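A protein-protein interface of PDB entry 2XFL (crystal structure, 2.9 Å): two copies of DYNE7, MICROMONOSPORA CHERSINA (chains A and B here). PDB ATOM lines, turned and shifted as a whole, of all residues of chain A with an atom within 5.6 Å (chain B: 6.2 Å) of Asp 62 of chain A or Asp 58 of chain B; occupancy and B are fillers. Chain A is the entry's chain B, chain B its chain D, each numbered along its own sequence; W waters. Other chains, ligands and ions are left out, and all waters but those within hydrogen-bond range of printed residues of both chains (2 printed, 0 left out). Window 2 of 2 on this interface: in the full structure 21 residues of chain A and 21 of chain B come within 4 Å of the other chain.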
ATOM      1  N   HIS A  60     -20.677  -5.561   5.348  1.00  0.00           N
ATOM      2  CA  HIS A  60     -22.016  -6.131   5.472  1.00  0.00           C
ATOM      3  C   HIS A  60     -22.936  -5.418   4.493  1.00  0.00           C
ATOM      4  O   HIS A  60     -22.683  -4.255   4.134  1.00  0.00           O
ATOM      5  CB  HIS A  60     -22.518  -5.955   6.900  1.00  0.00           C
ATOM      6  CG  HIS A  60     -23.774  -6.706   7.200  1.00  0.00           C
ATOM      7  ND1 HIS A  60     -25.014  -6.152   6.968  1.00  0.00           N
ATOM      8  CD2 HIS A  60     -23.945  -7.950   7.716  1.00  0.00           C
ATOM      9  CE1 HIS A  60     -25.899  -7.070   7.338  1.00  0.00           C
ATOM     10  NE2 HIS A  60     -25.305  -8.177   7.786  1.00  0.00           N
ATOM     11  N   ALA A  61     -23.973  -6.132   4.021  1.00  0.00           N
ATOM     12  CA  ALA A  61     -25.022  -5.595   3.143  1.00  0.00           C
ATOM     13  C   ALA A  61     -26.384  -6.236   3.488  1.00  0.00           C
ATOM     14  O   ALA A  61     -26.425  -7.397   3.889  1.00  0.00           O
ATOM     15  CB  ALA A  61     -24.661  -5.831   1.678  1.00  0.00           C
ATOM     16  N   ASP A  62     -27.480  -5.471   3.374  1.00  0.00           N
ATOM     17  CA  ASP A  62     -28.840  -5.993   3.523  1.00  0.00           C
ATOM     18  C   ASP A  62     -29.635  -5.604   2.284  1.00  0.00           C
ATOM     19  O   ASP A  62     -29.559  -4.437   1.884  1.00  0.00           O
ATOM     20  CB  ASP A  62     -29.508  -5.352   4.736  1.00  0.00           C
ATOM     21  CG  ASP A  62     -28.811  -5.698   6.000  1.00  0.00           C
ATOM     22  OD1 ASP A  62     -28.993  -6.847   6.474  1.00  0.00           O
ATOM     23  OD2 ASP A  62     -28.083  -4.811   6.532  1.00  0.00           O
ATOM     24  N   PHE A  63     -30.391  -6.524   1.897  1.00  0.00           N
ATOM     25  CA  PHE A  63     -31.029  -6.260   0.621  1.00  0.00           C
ATOM     26  C   PHE A  63     -32.574  -6.238   0.738  1.00  0.00           C
ATOM     27  O   PHE A  63     -33.180  -7.254   1.089  1.00  0.00           O
ATOM     28  CB  PHE A  63     -30.502  -7.257  -0.448  1.00  0.00           C
ATOM     29  CG  PHE A  63     -28.983  -7.428  -0.546  1.00  0.00           C
ATOM     30  CD1 PHE A  63     -28.219  -6.593  -1.344  1.00  0.00           C
ATOM     31  CD2 PHE A  63     -28.334  -8.447   0.137  1.00  0.00           C
ATOM     32  CE1 PHE A  63     -26.839  -6.759  -1.437  1.00  0.00           C
ATOM     33  CE2 PHE A  63     -26.947  -8.590   0.059  1.00  0.00           C
ATOM     34  CZ  PHE A  63     -26.220  -7.761  -0.751  1.00  0.00           C
ATOM     35  N   TYR A  64     -33.229  -5.087   0.254  1.00  0.00           N
ATOM     36  CA  TYR A  64     -34.662  -4.807   0.461  1.00  0.00           C
ATOM     37  C   TYR A  64     -35.497  -4.812  -0.805  1.00  0.00           C
ATOM     38  O   TYR A  64     -36.652  -5.263  -0.764  1.00  0.00           O
ATOM     39  CB  TYR A  64     -34.909  -3.465   1.225  1.00  0.00           C
ATOM     40  CG  TYR A  64     -34.107  -3.304   2.500  1.00  0.00           C
ATOM     41  CD1 TYR A  64     -34.400  -4.058   3.631  1.00  0.00           C
ATOM     42  CD2 TYR A  64     -33.009  -2.453   2.551  1.00  0.00           C
ATOM     43  CE1 TYR A  64     -33.613  -3.976   4.776  1.00  0.00           C
ATOM     44  CE2 TYR A  64     -32.220  -2.357   3.695  1.00  0.00           C
ATOM     45  CZ  TYR A  64     -32.518  -3.130   4.799  1.00  0.00           C
ATOM     46  OH  TYR A  64     -31.745  -3.029   5.923  1.00  0.00           O
ATOM     47  N   LEU A 104     -32.970   0.199  -1.955  1.00  0.00           N
ATOM     48  CA  LEU A 104     -32.673  -1.122  -2.498  1.00  0.00           C
ATOM     49  C   LEU A 104     -31.973  -1.958  -1.439  1.00  0.00           C
ATOM     50  O   LEU A 104     -32.371  -3.099  -1.189  1.00  0.00           O
ATOM     51  CB  LEU A 104     -31.822  -1.020  -3.752  1.00  0.00           C
ATOM     52  CG  LEU A 104     -32.433  -0.239  -4.925  1.00  0.00           C
ATOM     53  CD1 LEU A 104     -31.423  -0.081  -6.044  1.00  0.00           C
ATOM     54  CD2 LEU A 104     -33.660  -0.931  -5.489  1.00  0.00           C
ATOM     55  N   ALA A 105     -30.886  -1.419  -0.823  1.00  0.00           N
ATOM     56  CA  ALA A 105     -30.111  -2.100   0.195  1.00  0.00           C
ATOM     57  C   ALA A 105     -29.510  -1.107   1.168  1.00  0.00           C
ATOM     58  O   ALA A 105     -29.684   0.091   1.023  1.00  0.00           O
ATOM     59  CB  ALA A 105     -29.008  -2.905  -0.463  1.00  0.00           C
ATOM     60  N   GLN A 106     -28.916  -1.661   2.278  1.00  0.00           N
ATOM     61  CA  GLN A 106     -28.085  -0.927   3.250  1.00  0.00           C
ATOM     62  C   GLN A 106     -26.839  -1.767   3.526  1.00  0.00           C
ATOM     63  O   GLN A 106     -26.890  -3.004   3.466  1.00  0.00           O
ATOM     64  CB  GLN A 106     -28.834  -0.696   4.566  1.00  0.00           C
ATOM     65  CG  GLN A 106     -30.007   0.233   4.421  1.00  0.00           C
ATOM     66  CD  GLN A 106     -30.616   0.565   5.747  1.00  0.00           C
ATOM     67  OE1 GLN A 106     -31.103  -0.297   6.505  1.00  0.00           O
ATOM     68  NE2 GLN A 106     -30.580   1.844   6.053  1.00  0.00           N
ATOM     69  N   GLY A 107     -25.732  -0.964   3.604  1.00  0.00           N
ATOM     70  CA  GLY A 107     -24.467  -1.632   3.864  1.00  0.00           C
ATOM     71  C   GLY A 107     -23.637  -0.979   4.943  1.00  0.00           C
ATOM     72  O   GLY A 107     -23.934   0.134   5.385  1.00  0.00           O
ATOM     73  N   ARG A 108     -22.693  -1.719   5.511  1.00  0.00           N
ATOM     74  CA  ARG A 108     -21.697  -1.163   6.429  1.00  0.00           C
ATOM     75  C   ARG A 108     -20.311  -1.664   6.028  1.00  0.00           C
ATOM     76  O   ARG A 108     -20.179  -2.619   5.238  1.00  0.00           O
ATOM     77  CB  ARG A 108     -21.996  -1.550   7.889  1.00  0.00           C
ATOM     78  CG  ARG A 108     -23.462  -1.478   8.301  1.00  0.00           C
ATOM     79  CD  ARG A 108     -23.658  -1.842   9.738  1.00  0.00           C
ATOM     80  NE  ARG A 108     -23.515  -3.279  10.002  1.00  0.00           N
ATOM     81  CZ  ARG A 108     -24.528  -4.131  10.013  1.00  0.00           C
ATOM     82  NH1 ARG A 108     -25.754  -3.714   9.739  1.00  0.00           N
ATOM     83  NH2 ARG A 108     -24.321  -5.414  10.277  1.00  0.00           N
ATOM     84  N   GLN B  29     -18.767 -16.841  -1.933  1.00  0.00           N
ATOM     85  CA  GLN B  29     -19.956 -17.337  -1.204  1.00  0.00           C
ATOM     86  C   GLN B  29     -21.039 -17.779  -2.173  1.00  0.00           C
ATOM     87  O   GLN B  29     -21.727 -18.765  -1.925  1.00  0.00           O
ATOM     88  CB  GLN B  29     -20.572 -16.235  -0.341  1.00  0.00           C
ATOM     89  CG  GLN B  29     -19.784 -15.866   0.850  1.00  0.00           C
ATOM     90  CD  GLN B  29     -20.520 -14.891   1.716  1.00  0.00           C
ATOM     91  OE1 GLN B  29     -21.644 -14.476   1.442  1.00  0.00           O
ATOM     92  NE2 GLN B  29     -19.894 -14.508   2.801  1.00  0.00           N
ATOM     93  N   THR B  56     -31.065 -13.157  -2.147  1.00  0.00           N
ATOM     94  CA  THR B  56     -30.159 -12.816  -1.039  1.00  0.00           C
ATOM     95  C   THR B  56     -30.812 -11.738  -0.133  1.00  0.00           C
ATOM     96  O   THR B  56     -31.228 -10.663  -0.620  1.00  0.00           O
ATOM     97  CB  THR B  56     -28.767 -12.432  -1.586  1.00  0.00           C
ATOM     98  OG1 THR B  56     -28.294 -13.507  -2.403  1.00  0.00           O
ATOM     99  CG2 THR B  56     -27.755 -12.153  -0.485  1.00  0.00           C
ATOM    100  N   VAL B  57     -30.919 -12.041   1.176  1.00  0.00           N
ATOM    101  CA  VAL B  57     -31.481 -11.123   2.181  1.00  0.00           C
ATOM    102  C   VAL B  57     -30.382 -10.182   2.739  1.00  0.00           C
ATOM    103  O   VAL B  57     -30.552  -8.945   2.775  1.00  0.00           O
ATOM    104  CB  VAL B  57     -32.260 -11.879   3.281  1.00  0.00           C
ATOM    105  CG1 VAL B  57     -32.662 -10.953   4.406  1.00  0.00           C
ATOM    106  CG2 VAL B  57     -33.490 -12.544   2.695  1.00  0.00           C
ATOM    107  N   ASP B  58     -29.247 -10.789   3.124  1.00  0.00           N
ATOM    108  CA  ASP B  58     -28.058 -10.118   3.629  1.00  0.00           C
ATOM    109  C   ASP B  58     -26.802 -10.948   3.390  1.00  0.00           C
ATOM    110  O   ASP B  58     -26.890 -12.126   3.059  1.00  0.00           O
ATOM    111  CB  ASP B  58     -28.212  -9.791   5.117  1.00  0.00           C
ATOM    112  CG  ASP B  58     -28.641 -10.954   5.961  1.00  0.00           C
ATOM    113  OD1 ASP B  58     -27.825 -11.884   6.142  1.00  0.00           O
ATOM    114  OD2 ASP B  58     -29.789 -10.928   6.466  1.00  0.00           O
ATOM    115  N   CYS B  59     -25.635 -10.328   3.523  1.00  0.00           N
ATOM    116  CA  CYS B  59     -24.360 -11.026   3.518  1.00  0.00           C
ATOM    117  C   CYS B  59     -23.367 -10.251   4.370  1.00  0.00           C
ATOM    118  O   CYS B  59     -23.492  -9.034   4.528  1.00  0.00           O
ATOM    119  CB  CYS B  59     -23.845 -11.225   2.099  1.00  0.00           C
ATOM    120  SG  CYS B  59     -23.459  -9.689   1.257  1.00  0.00           S
ATOM    121  N   HIS B  60     -22.384 -10.970   4.915  1.00  0.00           N
ATOM    122  CA  HIS B  60     -21.357 -10.435   5.776  1.00  0.00           C
ATOM    123  C   HIS B  60     -20.057 -11.166   5.520  1.00  0.00           C
ATOM    124  O   HIS B  60     -20.081 -12.339   5.182  1.00  0.00           O
ATOM    125  CB  HIS B  60     -21.787 -10.564   7.253  1.00  0.00           C
ATOM    126  CG  HIS B  60     -20.939  -9.785   8.189  1.00  0.00           C
ATOM    127  ND1 HIS B  60     -19.808 -10.334   8.732  1.00  0.00           N
ATOM    128  CD2 HIS B  60     -21.076  -8.521   8.642  1.00  0.00           C
ATOM    129  CE1 HIS B  60     -19.298  -9.403   9.523  1.00  0.00           C
ATOM    130  NE2 HIS B  60     -20.027  -8.293   9.501  1.00  0.00           N
ATOM    131  N   ARG B  86     -36.616 -19.345   4.618  1.00  0.00           N
ATOM    132  CA  ARG B  86     -35.241 -18.800   4.754  1.00  0.00           C
ATOM    133  C   ARG B  86     -34.136 -19.795   5.103  1.00  0.00           C
ATOM    134  O   ARG B  86     -34.374 -20.762   5.826  1.00  0.00           O
ATOM    135  CB  ARG B  86     -35.214 -17.674   5.787  1.00  0.00           C
ATOM    136  CG  ARG B  86     -35.764 -16.345   5.283  1.00  0.00           C
ATOM    137  CD  ARG B  86     -36.363 -15.608   6.449  1.00  0.00           C
ATOM    138  NE  ARG B  86     -36.404 -14.168   6.233  1.00  0.00           N
ATOM    139  CZ  ARG B  86     -35.397 -13.338   6.497  1.00  0.00           C
ATOM    140  NH1 ARG B  86     -34.239 -13.809   6.951  1.00  0.00           N
ATOM    141  NH2 ARG B  86     -35.544 -12.030   6.316  1.00  0.00           N
ATOM    142  N   ARG B 108     -20.937 -14.806   6.263  1.00  0.00           N
ATOM    143  CA  ARG B 108     -22.284 -15.348   6.445  1.00  0.00           C
ATOM    144  C   ARG B 108     -23.195 -14.867   5.295  1.00  0.00           C
ATOM    145  O   ARG B 108     -22.846 -13.932   4.567  1.00  0.00           O
ATOM    146  CB  ARG B 108     -22.896 -14.929   7.775  1.00  0.00           C
ATOM    147  CG  ARG B 108     -21.996 -14.953   8.961  1.00  0.00           C
ATOM    148  CD  ARG B 108     -22.760 -14.514  10.185  1.00  0.00           C
ATOM    149  NE  ARG B 108     -22.929 -13.060  10.293  1.00  0.00           N
ATOM    150  CZ  ARG B 108     -22.057 -12.242  10.874  1.00  0.00           C
ATOM    151  NH1 ARG B 108     -20.906 -12.710  11.343  1.00  0.00           N
ATOM    152  NH2 ARG B 108     -22.315 -10.946  10.965  1.00  0.00           N
ATOM    153  N   GLN B 109     -24.367 -15.489   5.143  1.00  0.00           N
ATOM    154  CA  GLN B 109     -25.324 -15.084   4.131  1.00  0.00           C
ATOM    155  C   GLN B 109     -26.692 -15.669   4.454  1.00  0.00           C
ATOM    156  O   GLN B 109     -26.779 -16.780   5.027  1.00  0.00           O
ATOM    157  CB  GLN B 109     -24.851 -15.591   2.791  1.00  0.00           C
ATOM    158  CG  GLN B 109     -25.432 -14.856   1.625  1.00  0.00           C
ATOM    159  CD  GLN B 109     -25.110 -15.635   0.405  1.00  0.00           C
ATOM    160  OE1 GLN B 109     -25.781 -16.631   0.107  1.00  0.00           O
ATOM    161  NE2 GLN B 109     -24.019 -15.250  -0.260  1.00  0.00           N
ATOM    162  N   THR B 110     -27.759 -14.912   4.105  1.00  0.00           N
ATOM    163  CA  THR B 110     -29.154 -15.330   4.258  1.00  0.00           C
ATOM    164  C   THR B 110     -29.824 -15.292   2.920  1.00  0.00           C
ATOM    165  O   THR B 110     -29.689 -14.318   2.175  1.00  0.00           O
ATOM    166  CB  THR B 110     -29.885 -14.510   5.322  1.00  0.00           C
ATOM    167  OG1 THR B 110     -29.071 -14.453   6.504  1.00  0.00           O
ATOM    168  CG2 THR B 110     -31.267 -15.087   5.669  1.00  0.00           C
ATOM    169  N   VAL B 111     -30.557 -16.338   2.614  1.00  0.00           N
ATOM    170  CA  VAL B 111     -31.211 -16.503   1.321  1.00  0.00           C
ATOM    171  C   VAL B 111     -32.702 -16.840   1.568  1.00  0.00           C
ATOM    172  O   VAL B 111     -33.005 -17.653   2.429  1.00  0.00           O
ATOM    173  CB  VAL B 111     -30.437 -17.570   0.472  1.00  0.00           C
ATOM    174  CG1 VAL B 111     -31.349 -18.305  -0.489  1.00  0.00           C
ATOM    175  CG2 VAL B 111     -29.277 -16.947  -0.293  1.00  0.00           C
HETATM  176  O   HOH W   1     -33.293  -8.934  -1.950  1.00  0.00           O
HETATM  177  O   HOH W   2     -25.005 -11.013   8.868  1.00  0.00           O
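The backbone NH (N) of Ala 61 of chain A sits at hydrogen-bond distance from the backbone carbonyl oxygen (O) of Cys 59 of chain B (3.0 Å).
The backbone NH (N) of Phe 63 of chain A is in hydrogen-bond range of the backbone carbonyl oxygen (O) of Val 57 of chain B (2.6 Å).
OD2 of Asp 62 of chain A sits close to ND1 of His 60 of chain A (3.4 Å).
N of Val 57 of chain B is in hydrogen-bond range of O of Thr 110 of chain B (2.8 Å).
The backbone NH (N) of Arg 108 of chain B lies within hydrogen-bond range of the backbone carbonyl oxygen (O) of His 60 of chain B (2.8 Å).
The side-chain carboxylate (OD1) of Asp 58 of chain B lies within hydrogen-bond range of the side-chain hydroxyl (OG1) of Thr 110 of chain B.
The backbone NH of Asp 62 of chain A lies within hydrogen-bond range of the backbone carbonyl oxygen of Gln 106 of chain A, 2.5 Å away.
The backbone carbonyl oxygen (O) of His 60 of chain A sits at hydrogen-bond distance from the backbone NH (N) of Arg 108 of chain A (2.9 Å).
Cys 59 of chain B touches His 60 of chain A.
His 60 of chain A touches His 60 of chain B (CD2 to CD2, 3.1 Å).
Ala 61 of chain A touches Asp 58 of chain B (O to CA, 3.2 Å).
O of Val 57 of chain B touches CA of Asp 62 of chain A (3.5 Å).
Asp 58 of chain B touches Asp 62 of chain A (CB to OD1, 3.3 Å).
Phe 63 of chain A touches Thr 56 of chain B.
CD2 of Phe 63 of chain A touches CA of Asp 58 of chain B, at 3.9 Å.
Phe 63 of chain A touches Cys 59 of chain B.
Of chain B, only Val 57 and Asp 58 come within 4 Å of Asp 62 of chain A.
Asp 58 of chain B touches just these residues of chain A: Ala 61, Asp 62 and Phe 63.
Of the printed residues of chain B, Phe 63 of chain A touches Thr 56 (3.5 Å), Val 57 (2.6 Å), Asp 58 (3.9 Å) and Cys 59 (3.8 Å).
Printed residues of chain A within 4 Å of Val 57 of chain B: Asp 62 and Phe 63.
Printed residues of chain A within 4 Å of Cys 59 of chain B: His 60 (3.4 Å), Ala 61 (3.0 Å) and Phe 63 (3.8 Å).
Of the printed residues of chain A, His 60 of chain B touches His 60 (3.1 Å).
Arg 108 of chain A touches none of the printed residues of chain B.
The nearest residue of chain B that does not touch Asp 62 of chain A is Cys 59 of chain B (5.2 Å).
The nearest printed residue of chain A that does not touch Cys 59 of chain B is Asp 62 of chain A (5.2 Å).
Printed residues of chain A that touch a printed residue of chain B: His 60, Ala 61, Asp 62 and Phe 63.
Hydrophobic or aromatic side chains of chain A that line the printed part of chain B: His 60 and Phe 63.
His 60 of chain B touches its own counterpart, His 60 of chain A.
2 positions are printed for both chains.
Of the 10 pairs that touch across the chains among the printed residues, 1 has its exchanged pair printed and touching as well.
Water W1 bridges O of Thr 56 of chain B and O of Phe 63 of chain A.
Water W2 bridges a ring nitrogen (NE2) of His 60 of chain A and the guanidinium group (NE) of Arg 108 of chain B.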
